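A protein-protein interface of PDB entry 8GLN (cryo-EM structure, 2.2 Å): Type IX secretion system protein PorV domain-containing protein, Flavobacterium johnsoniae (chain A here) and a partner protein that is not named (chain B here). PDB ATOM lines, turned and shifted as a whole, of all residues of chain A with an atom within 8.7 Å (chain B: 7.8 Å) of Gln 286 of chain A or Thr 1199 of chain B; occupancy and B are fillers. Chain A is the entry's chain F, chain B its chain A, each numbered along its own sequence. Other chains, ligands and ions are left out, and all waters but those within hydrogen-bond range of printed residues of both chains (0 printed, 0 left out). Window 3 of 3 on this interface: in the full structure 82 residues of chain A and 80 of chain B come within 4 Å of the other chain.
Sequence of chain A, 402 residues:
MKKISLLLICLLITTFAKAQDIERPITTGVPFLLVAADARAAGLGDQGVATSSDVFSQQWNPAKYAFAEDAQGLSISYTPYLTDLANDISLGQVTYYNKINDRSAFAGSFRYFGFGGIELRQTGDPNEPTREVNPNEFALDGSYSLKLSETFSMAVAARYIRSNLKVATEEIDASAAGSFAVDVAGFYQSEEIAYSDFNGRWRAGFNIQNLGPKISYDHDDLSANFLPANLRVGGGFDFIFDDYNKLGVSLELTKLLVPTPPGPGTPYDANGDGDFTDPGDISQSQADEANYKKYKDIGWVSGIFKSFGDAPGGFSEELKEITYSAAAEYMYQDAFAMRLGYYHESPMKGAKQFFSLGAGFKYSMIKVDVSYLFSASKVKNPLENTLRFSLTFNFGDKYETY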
ATOM      1  N   PRO A 264     -17.046  10.191 -27.430  1.00  0.00           N
ATOM      2  CA  PRO A 264     -17.983  11.291 -27.707  1.00  0.00           C
ATOM      3  C   PRO A 264     -17.954  12.405 -26.671  1.00  0.00           C
ATOM      4  O   PRO A 264     -17.735  13.570 -27.016  1.00  0.00           O
ATOM      5  CB  PRO A 264     -19.352  10.588 -27.717  1.00  0.00           C
ATOM      6  CG  PRO A 264     -19.067   9.116 -27.384  1.00  0.00           C
ATOM      7  CD  PRO A 264     -17.648   8.895 -27.766  1.00  0.00           C
ATOM      8  N   PRO A 267     -18.806  14.878 -19.529  1.00  0.00           N
ATOM      9  CA  PRO A 267     -18.306  15.846 -18.546  1.00  0.00           C
ATOM     10  C   PRO A 267     -18.859  15.595 -17.146  1.00  0.00           C
ATOM     11  O   PRO A 267     -18.559  16.371 -16.239  1.00  0.00           O
ATOM     12  CB  PRO A 267     -18.793  17.193 -19.086  1.00  0.00           C
ATOM     13  CG  PRO A 267     -19.915  16.882 -20.015  1.00  0.00           C
ATOM     14  CD  PRO A 267     -19.875  15.430 -20.379  1.00  0.00           C
ATOM     15  N   SER A 283     -17.922  24.209 -24.576  1.00  0.00           N
ATOM     16  CA  SER A 283     -17.887  24.159 -26.033  1.00  0.00           C
ATOM     17  C   SER A 283     -17.929  22.720 -26.536  1.00  0.00           C
ATOM     18  O   SER A 283     -18.397  21.821 -25.837  1.00  0.00           O
ATOM     19  CB  SER A 283     -16.637  24.864 -26.563  1.00  0.00           C
ATOM     20  OG  SER A 283     -16.525  24.715 -27.968  1.00  0.00           O
ATOM     21  N   GLN A 284     -17.437  22.508 -27.755  1.00  0.00           N
ATOM     22  CA  GLN A 284     -17.412  21.177 -28.354  1.00  0.00           C
ATOM     23  C   GLN A 284     -16.087  20.467 -28.084  1.00  0.00           C
ATOM     24  O   GLN A 284     -16.065  19.380 -27.501  1.00  0.00           O
ATOM     25  CB  GLN A 284     -17.677  21.272 -29.861  1.00  0.00           C
ATOM     26  CG  GLN A 284     -17.658  19.931 -30.577  1.00  0.00           C
ATOM     27  CD  GLN A 284     -18.745  18.996 -30.087  1.00  0.00           C
ATOM     28  OE1 GLN A 284     -19.880  19.412 -29.853  1.00  0.00           O
ATOM     29  NE2 GLN A 284     -18.403  17.723 -29.930  1.00  0.00           N
ATOM     30  N   SER A 285     -14.976  21.073 -28.505  1.00  0.00           N
ATOM     31  CA  SER A 285     -13.666  20.485 -28.259  1.00  0.00           C
ATOM     32  C   SER A 285     -13.197  20.678 -26.824  1.00  0.00           C
ATOM     33  O   SER A 285     -12.311  19.944 -26.374  1.00  0.00           O
ATOM     34  CB  SER A 285     -12.632  21.074 -29.222  1.00  0.00           C
ATOM     35  OG  SER A 285     -12.892  20.672 -30.556  1.00  0.00           O
ATOM     36  N   GLN A 286     -13.769  21.644 -26.101  1.00  0.00           N
ATOM     37  CA  GLN A 286     -13.402  21.832 -24.701  1.00  0.00           C
ATOM     38  C   GLN A 286     -13.776  20.615 -23.867  1.00  0.00           C
ATOM     39  O   GLN A 286     -13.010  20.190 -22.995  1.00  0.00           O
ATOM     40  CB  GLN A 286     -14.071  23.089 -24.145  1.00  0.00           C
ATOM     41  CG  GLN A 286     -13.525  24.388 -24.708  1.00  0.00           C
ATOM     42  CD  GLN A 286     -14.149  25.608 -24.061  1.00  0.00           C
ATOM     43  OE1 GLN A 286     -15.052  25.493 -23.233  1.00  0.00           O
ATOM     44  NE2 GLN A 286     -13.667  26.788 -24.434  1.00  0.00           N
ATOM     45  N   ALA A 287     -14.957  20.043 -24.118  1.00  0.00           N
ATOM     46  CA  ALA A 287     -15.370  18.848 -23.389  1.00  0.00           C
ATOM     47  C   ALA A 287     -14.438  17.678 -23.677  1.00  0.00           C
ATOM     48  O   ALA A 287     -14.058  16.940 -22.761  1.00  0.00           O
ATOM     49  CB  ALA A 287     -16.812  18.488 -23.743  1.00  0.00           C
ATOM     50  N   ASP A 288     -14.061  17.493 -24.944  1.00  0.00           N
ATOM     51  CA  ASP A 288     -13.141  16.416 -25.296  1.00  0.00           C
ATOM     52  C   ASP A 288     -11.781  16.614 -24.638  1.00  0.00           C
ATOM     53  O   ASP A 288     -11.186  15.659 -24.122  1.00  0.00           O
ATOM     54  CB  ASP A 288     -12.994  16.331 -26.816  1.00  0.00           C
ATOM     55  CG  ASP A 288     -12.695  14.926 -27.297  1.00  0.00           C
ATOM     56  OD1 ASP A 288     -11.711  14.326 -26.815  1.00  0.00           O
ATOM     57  OD2 ASP A 288     -13.443  14.421 -28.160  1.00  0.00           O
ATOM     58  N   GLU A 289     -11.274  17.849 -24.648  1.00  0.00           N
ATOM     59  CA  GLU A 289      -9.984  18.120 -24.025  1.00  0.00           C
ATOM     60  C   GLU A 289     -10.035  17.885 -22.520  1.00  0.00           C
ATOM     61  O   GLU A 289      -9.102  17.316 -21.946  1.00  0.00           O
ATOM     62  CB  GLU A 289      -9.538  19.548 -24.333  1.00  0.00           C
ATOM     63  CG  GLU A 289      -8.224  19.933 -23.674  1.00  0.00           C
ATOM     64  CD  GLU A 289      -7.642  21.216 -24.230  1.00  0.00           C
ATOM     65  OE1 GLU A 289      -8.269  21.818 -25.126  1.00  0.00           O
ATOM     66  OE2 GLU A 289      -6.555  21.621 -23.768  1.00  0.00           O
ATOM     67  N   ALA A 290     -11.118  18.310 -21.863  1.00  0.00           N
ATOM     68  CA  ALA A 290     -11.253  18.075 -20.429  1.00  0.00           C
ATOM     69  C   ALA A 290     -11.361  16.587 -20.119  1.00  0.00           C
ATOM     70  O   ALA A 290     -10.793  16.108 -19.128  1.00  0.00           O
ATOM     71  CB  ALA A 290     -12.466  18.827 -19.885  1.00  0.00           C
ATOM     72  N   ASN A 291     -12.096  15.840 -20.946  1.00  0.00           N
ATOM     73  CA  ASN A 291     -12.212  14.401 -20.740  1.00  0.00           C
ATOM     74  C   ASN A 291     -10.863  13.711 -20.890  1.00  0.00           C
ATOM     75  O   ASN A 291     -10.517  12.828 -20.096  1.00  0.00           O
ATOM     76  CB  ASN A 291     -13.231  13.816 -21.718  1.00  0.00           C
ATOM     77  CG  ASN A 291     -14.664  14.034 -21.267  1.00  0.00           C
ATOM     78  OD1 ASN A 291     -15.605  13.583 -21.919  1.00  0.00           O
ATOM     79  ND2 ASN A 291     -14.835  14.726 -20.148  1.00  0.00           N
ATOM     80  N   TYR A 292     -10.083  14.103 -21.902  1.00  0.00           N
ATOM     81  CA  TYR A 292      -8.753  13.523 -22.065  1.00  0.00           C
ATOM     82  C   TYR A 292      -7.830  13.931 -20.921  1.00  0.00           C
ATOM     83  O   TYR A 292      -6.984  13.142 -20.487  1.00  0.00           O
ATOM     84  CB  TYR A 292      -8.157  13.930 -23.412  1.00  0.00           C
ATOM     85  CG  TYR A 292      -6.964  13.094 -23.811  1.00  0.00           C
ATOM     86  CD1 TYR A 292      -7.124  11.780 -24.234  1.00  0.00           C
ATOM     87  CD2 TYR A 292      -5.678  13.611 -23.755  1.00  0.00           C
ATOM     88  CE1 TYR A 292      -6.038  11.009 -24.597  1.00  0.00           C
ATOM     89  CE2 TYR A 292      -4.584  12.847 -24.115  1.00  0.00           C
ATOM     90  CZ  TYR A 292      -4.770  11.547 -24.535  1.00  0.00           C
ATOM     91  OH  TYR A 292      -3.685  10.782 -24.897  1.00  0.00           O
ATOM     92  N   LYS A 293      -7.979  15.162 -20.427  1.00  0.00           N
ATOM     93  CA  LYS A 293      -7.236  15.603 -19.250  1.00  0.00           C
ATOM     94  C   LYS A 293      -7.522  14.708 -18.054  1.00  0.00           C
ATOM     95  O   LYS A 293      -6.603  14.270 -17.354  1.00  0.00           O
ATOM     96  CB  LYS A 293      -7.605  17.051 -18.930  1.00  0.00           C
ATOM     97  CG  LYS A 293      -6.645  17.776 -18.008  1.00  0.00           C
ATOM     98  CD  LYS A 293      -6.487  19.227 -18.423  1.00  0.00           C
ATOM     99  CE  LYS A 293      -5.512  19.949 -17.515  1.00  0.00           C
ATOM    100  NZ  LYS A 293      -4.842  21.086 -18.202  1.00  0.00           N
ATOM    101  N   LYS A 294      -8.802  14.436 -17.799  1.00  0.00           N
ATOM    102  CA  LYS A 294      -9.164  13.578 -16.675  1.00  0.00           C
ATOM    103  C   LYS A 294      -8.662  12.153 -16.880  1.00  0.00           C
ATOM    104  O   LYS A 294      -8.178  11.519 -15.936  1.00  0.00           O
ATOM    105  CB  LYS A 294     -10.678  13.592 -16.467  1.00  0.00           C
ATOM    106  CG  LYS A 294     -11.210  14.897 -15.898  1.00  0.00           C
ATOM    107  CD  LYS A 294     -12.668  14.772 -15.488  1.00  0.00           C
ATOM    108  CE  LYS A 294     -13.583  14.727 -16.699  1.00  0.00           C
ATOM    109  NZ  LYS A 294     -15.019  14.755 -16.310  1.00  0.00           N
ATOM    110  N   GLU B 942      -1.881  17.928 -28.998  1.00  0.00           N
ATOM    111  CA  GLU B 942      -2.412  19.282 -28.876  1.00  0.00           C
ATOM    112  C   GLU B 942      -2.700  19.887 -30.243  1.00  0.00           C
ATOM    113  O   GLU B 942      -3.757  20.493 -30.450  1.00  0.00           O
ATOM    114  CB  GLU B 942      -1.436  20.159 -28.093  1.00  0.00           C
ATOM    115  CG  GLU B 942      -1.841  21.620 -28.018  1.00  0.00           C
ATOM    116  CD  GLU B 942      -0.768  22.489 -27.397  1.00  0.00           C
ATOM    117  OE1 GLU B 942      -0.192  22.078 -26.369  1.00  0.00           O
ATOM    118  OE2 GLU B 942      -0.500  23.582 -27.938  1.00  0.00           O
ATOM    119  N   ARG B1196      -7.569  26.680 -33.972  1.00  0.00           N
ATOM    120  CA  ARG B1196      -7.792  25.701 -32.920  1.00  0.00           C
ATOM    121  C   ARG B1196      -7.435  26.322 -31.578  1.00  0.00           C
ATOM    122  O   ARG B1196      -6.328  26.843 -31.404  1.00  0.00           O
ATOM    123  CB  ARG B1196      -6.964  24.437 -33.156  1.00  0.00           C
ATOM    124  CG  ARG B1196      -7.141  23.376 -32.082  1.00  0.00           C
ATOM    125  CD  ARG B1196      -6.424  22.085 -32.447  1.00  0.00           C
ATOM    126  NE  ARG B1196      -7.243  21.208 -33.276  1.00  0.00           N
ATOM    127  CZ  ARG B1196      -8.333  20.576 -32.862  1.00  0.00           C
ATOM    128  NH1 ARG B1196      -8.762  20.678 -31.614  1.00  0.00           N
ATOM    129  NH2 ARG B1196      -9.008  19.817 -33.720  1.00  0.00           N
ATOM    130  N   GLU B1197      -8.371  26.266 -30.636  1.00  0.00           N
ATOM    131  CA  GLU B1197      -8.181  26.822 -29.304  1.00  0.00           C
ATOM    132  C   GLU B1197      -7.843  25.708 -28.323  1.00  0.00           C
ATOM    133  O   GLU B1197      -8.542  24.692 -28.264  1.00  0.00           O
ATOM    134  CB  GLU B1197      -9.431  27.570 -28.839  1.00  0.00           C
ATOM    135  CG  GLU B1197     -10.079  28.424 -29.907  1.00  0.00           C
ATOM    136  CD  GLU B1197      -9.730  29.889 -29.762  1.00  0.00           C
ATOM    137  OE1 GLU B1197      -8.910  30.216 -28.879  1.00  0.00           O
ATOM    138  OE2 GLU B1197     -10.273  30.713 -30.526  1.00  0.00           O
ATOM    139  N   VAL B1198      -6.771  25.903 -27.562  1.00  0.00           N
ATOM    140  CA  VAL B1198      -6.378  25.000 -26.488  1.00  0.00           C
ATOM    141  C   VAL B1198      -6.623  25.734 -25.178  1.00  0.00           C
ATOM    142  O   VAL B1198      -6.139  26.857 -24.988  1.00  0.00           O
ATOM    143  CB  VAL B1198      -4.912  24.562 -26.620  1.00  0.00           C
ATOM    144  CG1 VAL B1198      -4.664  23.300 -25.816  1.00  0.00           C
ATOM    145  CG2 VAL B1198      -4.551  24.345 -28.081  1.00  0.00           C
ATOM    146  N   THR B1199      -7.375  25.108 -24.275  1.00  0.00           N
ATOM    147  CA  THR B1199      -7.886  25.791 -23.090  1.00  0.00           C
ATOM    148  C   THR B1199      -7.013  25.600 -21.856  1.00  0.00           C
ATOM    149  O   THR B1199      -6.572  26.583 -21.257  1.00  0.00           O
ATOM    150  CB  THR B1199      -9.315  25.321 -22.792  1.00  0.00           C
ATOM    151  OG1 THR B1199      -9.333  23.897 -22.641  1.00  0.00           O
ATOM    152  CG2 THR B1199     -10.247  25.718 -23.923  1.00  0.00           C
ATOM    153  N   ASN B1200      -6.755  24.356 -21.455  1.00  0.00           N
ATOM    154  CA  ASN B1200      -6.024  24.068 -20.220  1.00  0.00           C
ATOM    155  C   ASN B1200      -4.846  23.156 -20.551  1.00  0.00           C
ATOM    156  O   ASN B1200      -4.982  21.930 -20.573  1.00  0.00           O
ATOM    157  CB  ASN B1200      -6.947  23.449 -19.174  1.00  0.00           C
ATOM    158  CG  ASN B1200      -7.950  24.444 -18.624  1.00  0.00           C
ATOM    159  OD1 ASN B1200      -9.121  24.439 -19.003  1.00  0.00           O
ATOM    160  ND2 ASN B1200      -7.493  25.308 -17.725  1.00  0.00           N
ATOM    161  N   VAL B1201      -3.691  23.761 -20.801  1.00  0.00           N
ATOM    162  CA  VAL B1201      -2.477  23.026 -21.134  1.00  0.00           C
ATOM    163  C   VAL B1201      -1.732  22.691 -19.849  1.00  0.00           C
ATOM    164  O   VAL B1201      -1.546  23.556 -18.985  1.00  0.00           O
ATOM    165  CB  VAL B1201      -1.583  23.843 -22.081  1.00  0.00           C
ATOM    166  CG1 VAL B1201      -0.366  23.032 -22.492  1.00  0.00           C
ATOM    167  CG2 VAL B1201      -2.367  24.298 -23.294  1.00  0.00           C
ATOM    168  N   ASP B1202      -1.309  21.437 -19.717  1.00  0.00           N
ATOM    169  CA  ASP B1202      -0.414  21.069 -18.630  1.00  0.00           C
ATOM    170  C   ASP B1202       0.935  21.750 -18.821  1.00  0.00           C
ATOM    171  O   ASP B1202       1.476  21.781 -19.930  1.00  0.00           O
ATOM    172  CB  ASP B1202      -0.233  19.554 -18.567  1.00  0.00           C
ATOM    173  CG  ASP B1202      -1.515  18.829 -18.239  1.00  0.00           C
ATOM    174  OD1 ASP B1202      -2.512  19.510 -17.930  1.00  0.00           O
ATOM    175  OD2 ASP B1202      -1.527  17.582 -18.282  1.00  0.00           O
ATOM    176  N   THR B1208      -1.442  26.102 -15.583  1.00  0.00           N
ATOM    177  CA  THR B1208      -2.111  25.902 -16.858  1.00  0.00           C
ATOM    178  C   THR B1208      -2.060  27.192 -17.663  1.00  0.00           C
ATOM    179  O   THR B1208      -1.794  28.272 -17.131  1.00  0.00           O
ATOM    180  CB  THR B1208      -3.571  25.458 -16.679  1.00  0.00           C
ATOM    181  OG1 THR B1208      -4.232  26.334 -15.758  1.00  0.00           O
ATOM    182  CG2 THR B1208      -3.638  24.031 -16.154  1.00  0.00           C
ATOM    183  N   THR B1209      -2.316  27.064 -18.962  1.00  0.00           N
ATOM    184  CA  THR B1209      -2.341  28.215 -19.849  1.00  0.00           C
ATOM    185  C   THR B1209      -3.249  27.914 -21.030  1.00  0.00           C
ATOM    186  O   THR B1209      -3.581  26.760 -21.309  1.00  0.00           O
ATOM    187  CB  THR B1209      -0.936  28.588 -20.343  1.00  0.00           C
ATOM    188  OG1 THR B1209      -0.977  29.860 -21.000  1.00  0.00           O
ATOM    189  CG2 THR B1209      -0.409  27.541 -21.314  1.00  0.00           C
ATOM    190  N   ASN B1210      -3.656  28.976 -21.713  1.00  0.00           N
ATOM    191  CA  ASN B1210      -4.396  28.860 -22.957  1.00  0.00           C
ATOM    192  C   ASN B1210      -3.445  28.973 -24.142  1.00  0.00           C
ATOM    193  O   ASN B1210      -2.343  29.511 -24.040  1.00  0.00           O
ATOM    194  CB  ASN B1210      -5.478  29.936 -23.048  1.00  0.00           C
ATOM    195  CG  ASN B1210      -6.416  29.920 -21.863  1.00  0.00           C
ATOM    196  OD1 ASN B1210      -7.413  29.201 -21.856  1.00  0.00           O
ATOM    197  ND2 ASN B1210      -6.102  30.718 -20.849  1.00  0.00           N
ATOM    198  N   ALA B1211      -3.890  28.447 -25.279  1.00  0.00           N
ATOM    199  CA  ALA B1211      -3.123  28.540 -26.510  1.00  0.00           C
ATOM    200  C   ALA B1211      -4.092  28.610 -27.678  1.00  0.00           C
ATOM    201  O   ALA B1211      -5.244  28.182 -27.582  1.00  0.00           O
ATOM    202  CB  ALA B1211      -2.160  27.358 -26.671  1.00  0.00           C
ATOM    203  N   ARG B1212      -3.609  29.158 -28.787  1.00  0.00           N
ATOM    204  CA  ARG B1212      -4.435  29.369 -29.970  1.00  0.00           C
ATOM    205  C   ARG B1212      -3.592  29.050 -31.194  1.00  0.00           C
ATOM    206  O   ARG B1212      -2.708  29.829 -31.562  1.00  0.00           O
ATOM    207  CB  ARG B1212      -4.962  30.804 -30.014  1.00  0.00           C
ATOM    208  CG  ARG B1212      -6.205  31.012 -30.855  1.00  0.00           C
ATOM    209  CD  ARG B1212      -6.742  32.418 -30.651  1.00  0.00           C
ATOM    210  NE  ARG B1212      -7.926  32.694 -31.452  1.00  0.00           N
ATOM    211  CZ  ARG B1212      -7.958  33.533 -32.477  1.00  0.00           C
ATOM    212  NH1 ARG B1212      -6.877  34.185 -32.870  1.00  0.00           N
ATOM    213  NH2 ARG B1212      -9.105  33.728 -33.121  1.00  0.00           N
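OG1 of Thr 1199 of chain B is in hydrogen-bond range of OE1 of Glu 289 of chain A (3.4 Å). OD1 of Asp 1202 of chain B is in salt-bridge range of NZ of Lys 293 of chain A (2.8 Å). The side-chain amino group (NZ) of Lys 293 of chain A lies within hydrogen-bond range of the backbone carbonyl oxygen (O) of Asn 1200 of chain B, 2.5 Å away.
N of Val 1201 of chain B sits at hydrogen-bond distance from O of Thr 1209 of chain B, at 3.0 Å. The side-chain amide oxygen (OE1) of Gln 286 of chain A lies within hydrogen-bond range of the backbone NH (N) of Ser 283 of chain A (3.4 Å). O of Thr 1199 of chain B sits close to OD1 of Asn 1210 of chain B. The backbone NH (N) of Val 1198 of chain B lies within hydrogen-bond range of the backbone carbonyl oxygen (O) of Ala 1211 of chain B, at 2.7 Å.
Among the printed residues, merely in contact across the chains: Glu 289 of chain A with Val 1198 of chain B (3.3 Å), Glu 289 of chain A with Asn 1200 of chain B (3.6 Å), Gln 286 of chain A with Thr 1199 of chain B (3.6 Å), Lys 293 of chain A with Thr 1208 of chain B (3.8 Å) and Lys 293 of chain A with Val 1201 of chain B (3.9 Å).
Printed residues of chain B within 4 Å of Gln 286 of chain A: Thr 1199 (3.6 Å). Thr 1199 of chain B touches two residues of chain A. Of chain A, only Glu 289 (3.6 Å) and Lys 293 (2.5 Å) come within 4 Å of Asn 1200 of chain B. Printed residues of chain A within 4 Å of Asp 1202 of chain B: Lys 293 (2.8 Å). Of the printed residues of chain A, Thr 1208 of chain B touches Lys 293 (3.8 Å). Printed residues of chain A within 4 Å of Val 1198 of chain B: Glu 289 (3.3 Å). Printed residues of chain B within 4 Å of Lys 293 of chain A: Asn 1200 (2.5 Å), Val 1201 (3.9 Å), Asp 1202 (2.8 Å) and Thr 1208 (3.8 Å). Of the printed residues of chain B, Glu 289 of chain A touches Val 1198 (3.3 Å), Thr 1199 (3.4 Å) and Asn 1200 (3.6 Å). Asp 288 of chain A touches none of the printed residues of chain B. The nearest residue of chain B that does not touch Gln 286 of chain A is Glu 1197 of chain B (6.1 Å). The nearest residue of chain A that does not touch Thr 1199 of chain B is Ala 290 of chain A (5.9 Å).
Of the 13 printed residues of chain B, 6 touch a printed residue of chain A. Hydrophobic or aromatic side chains of chain B that line the printed part of chain A: Val 1198. Among the printed residues, 8 pairs touch across the chains.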
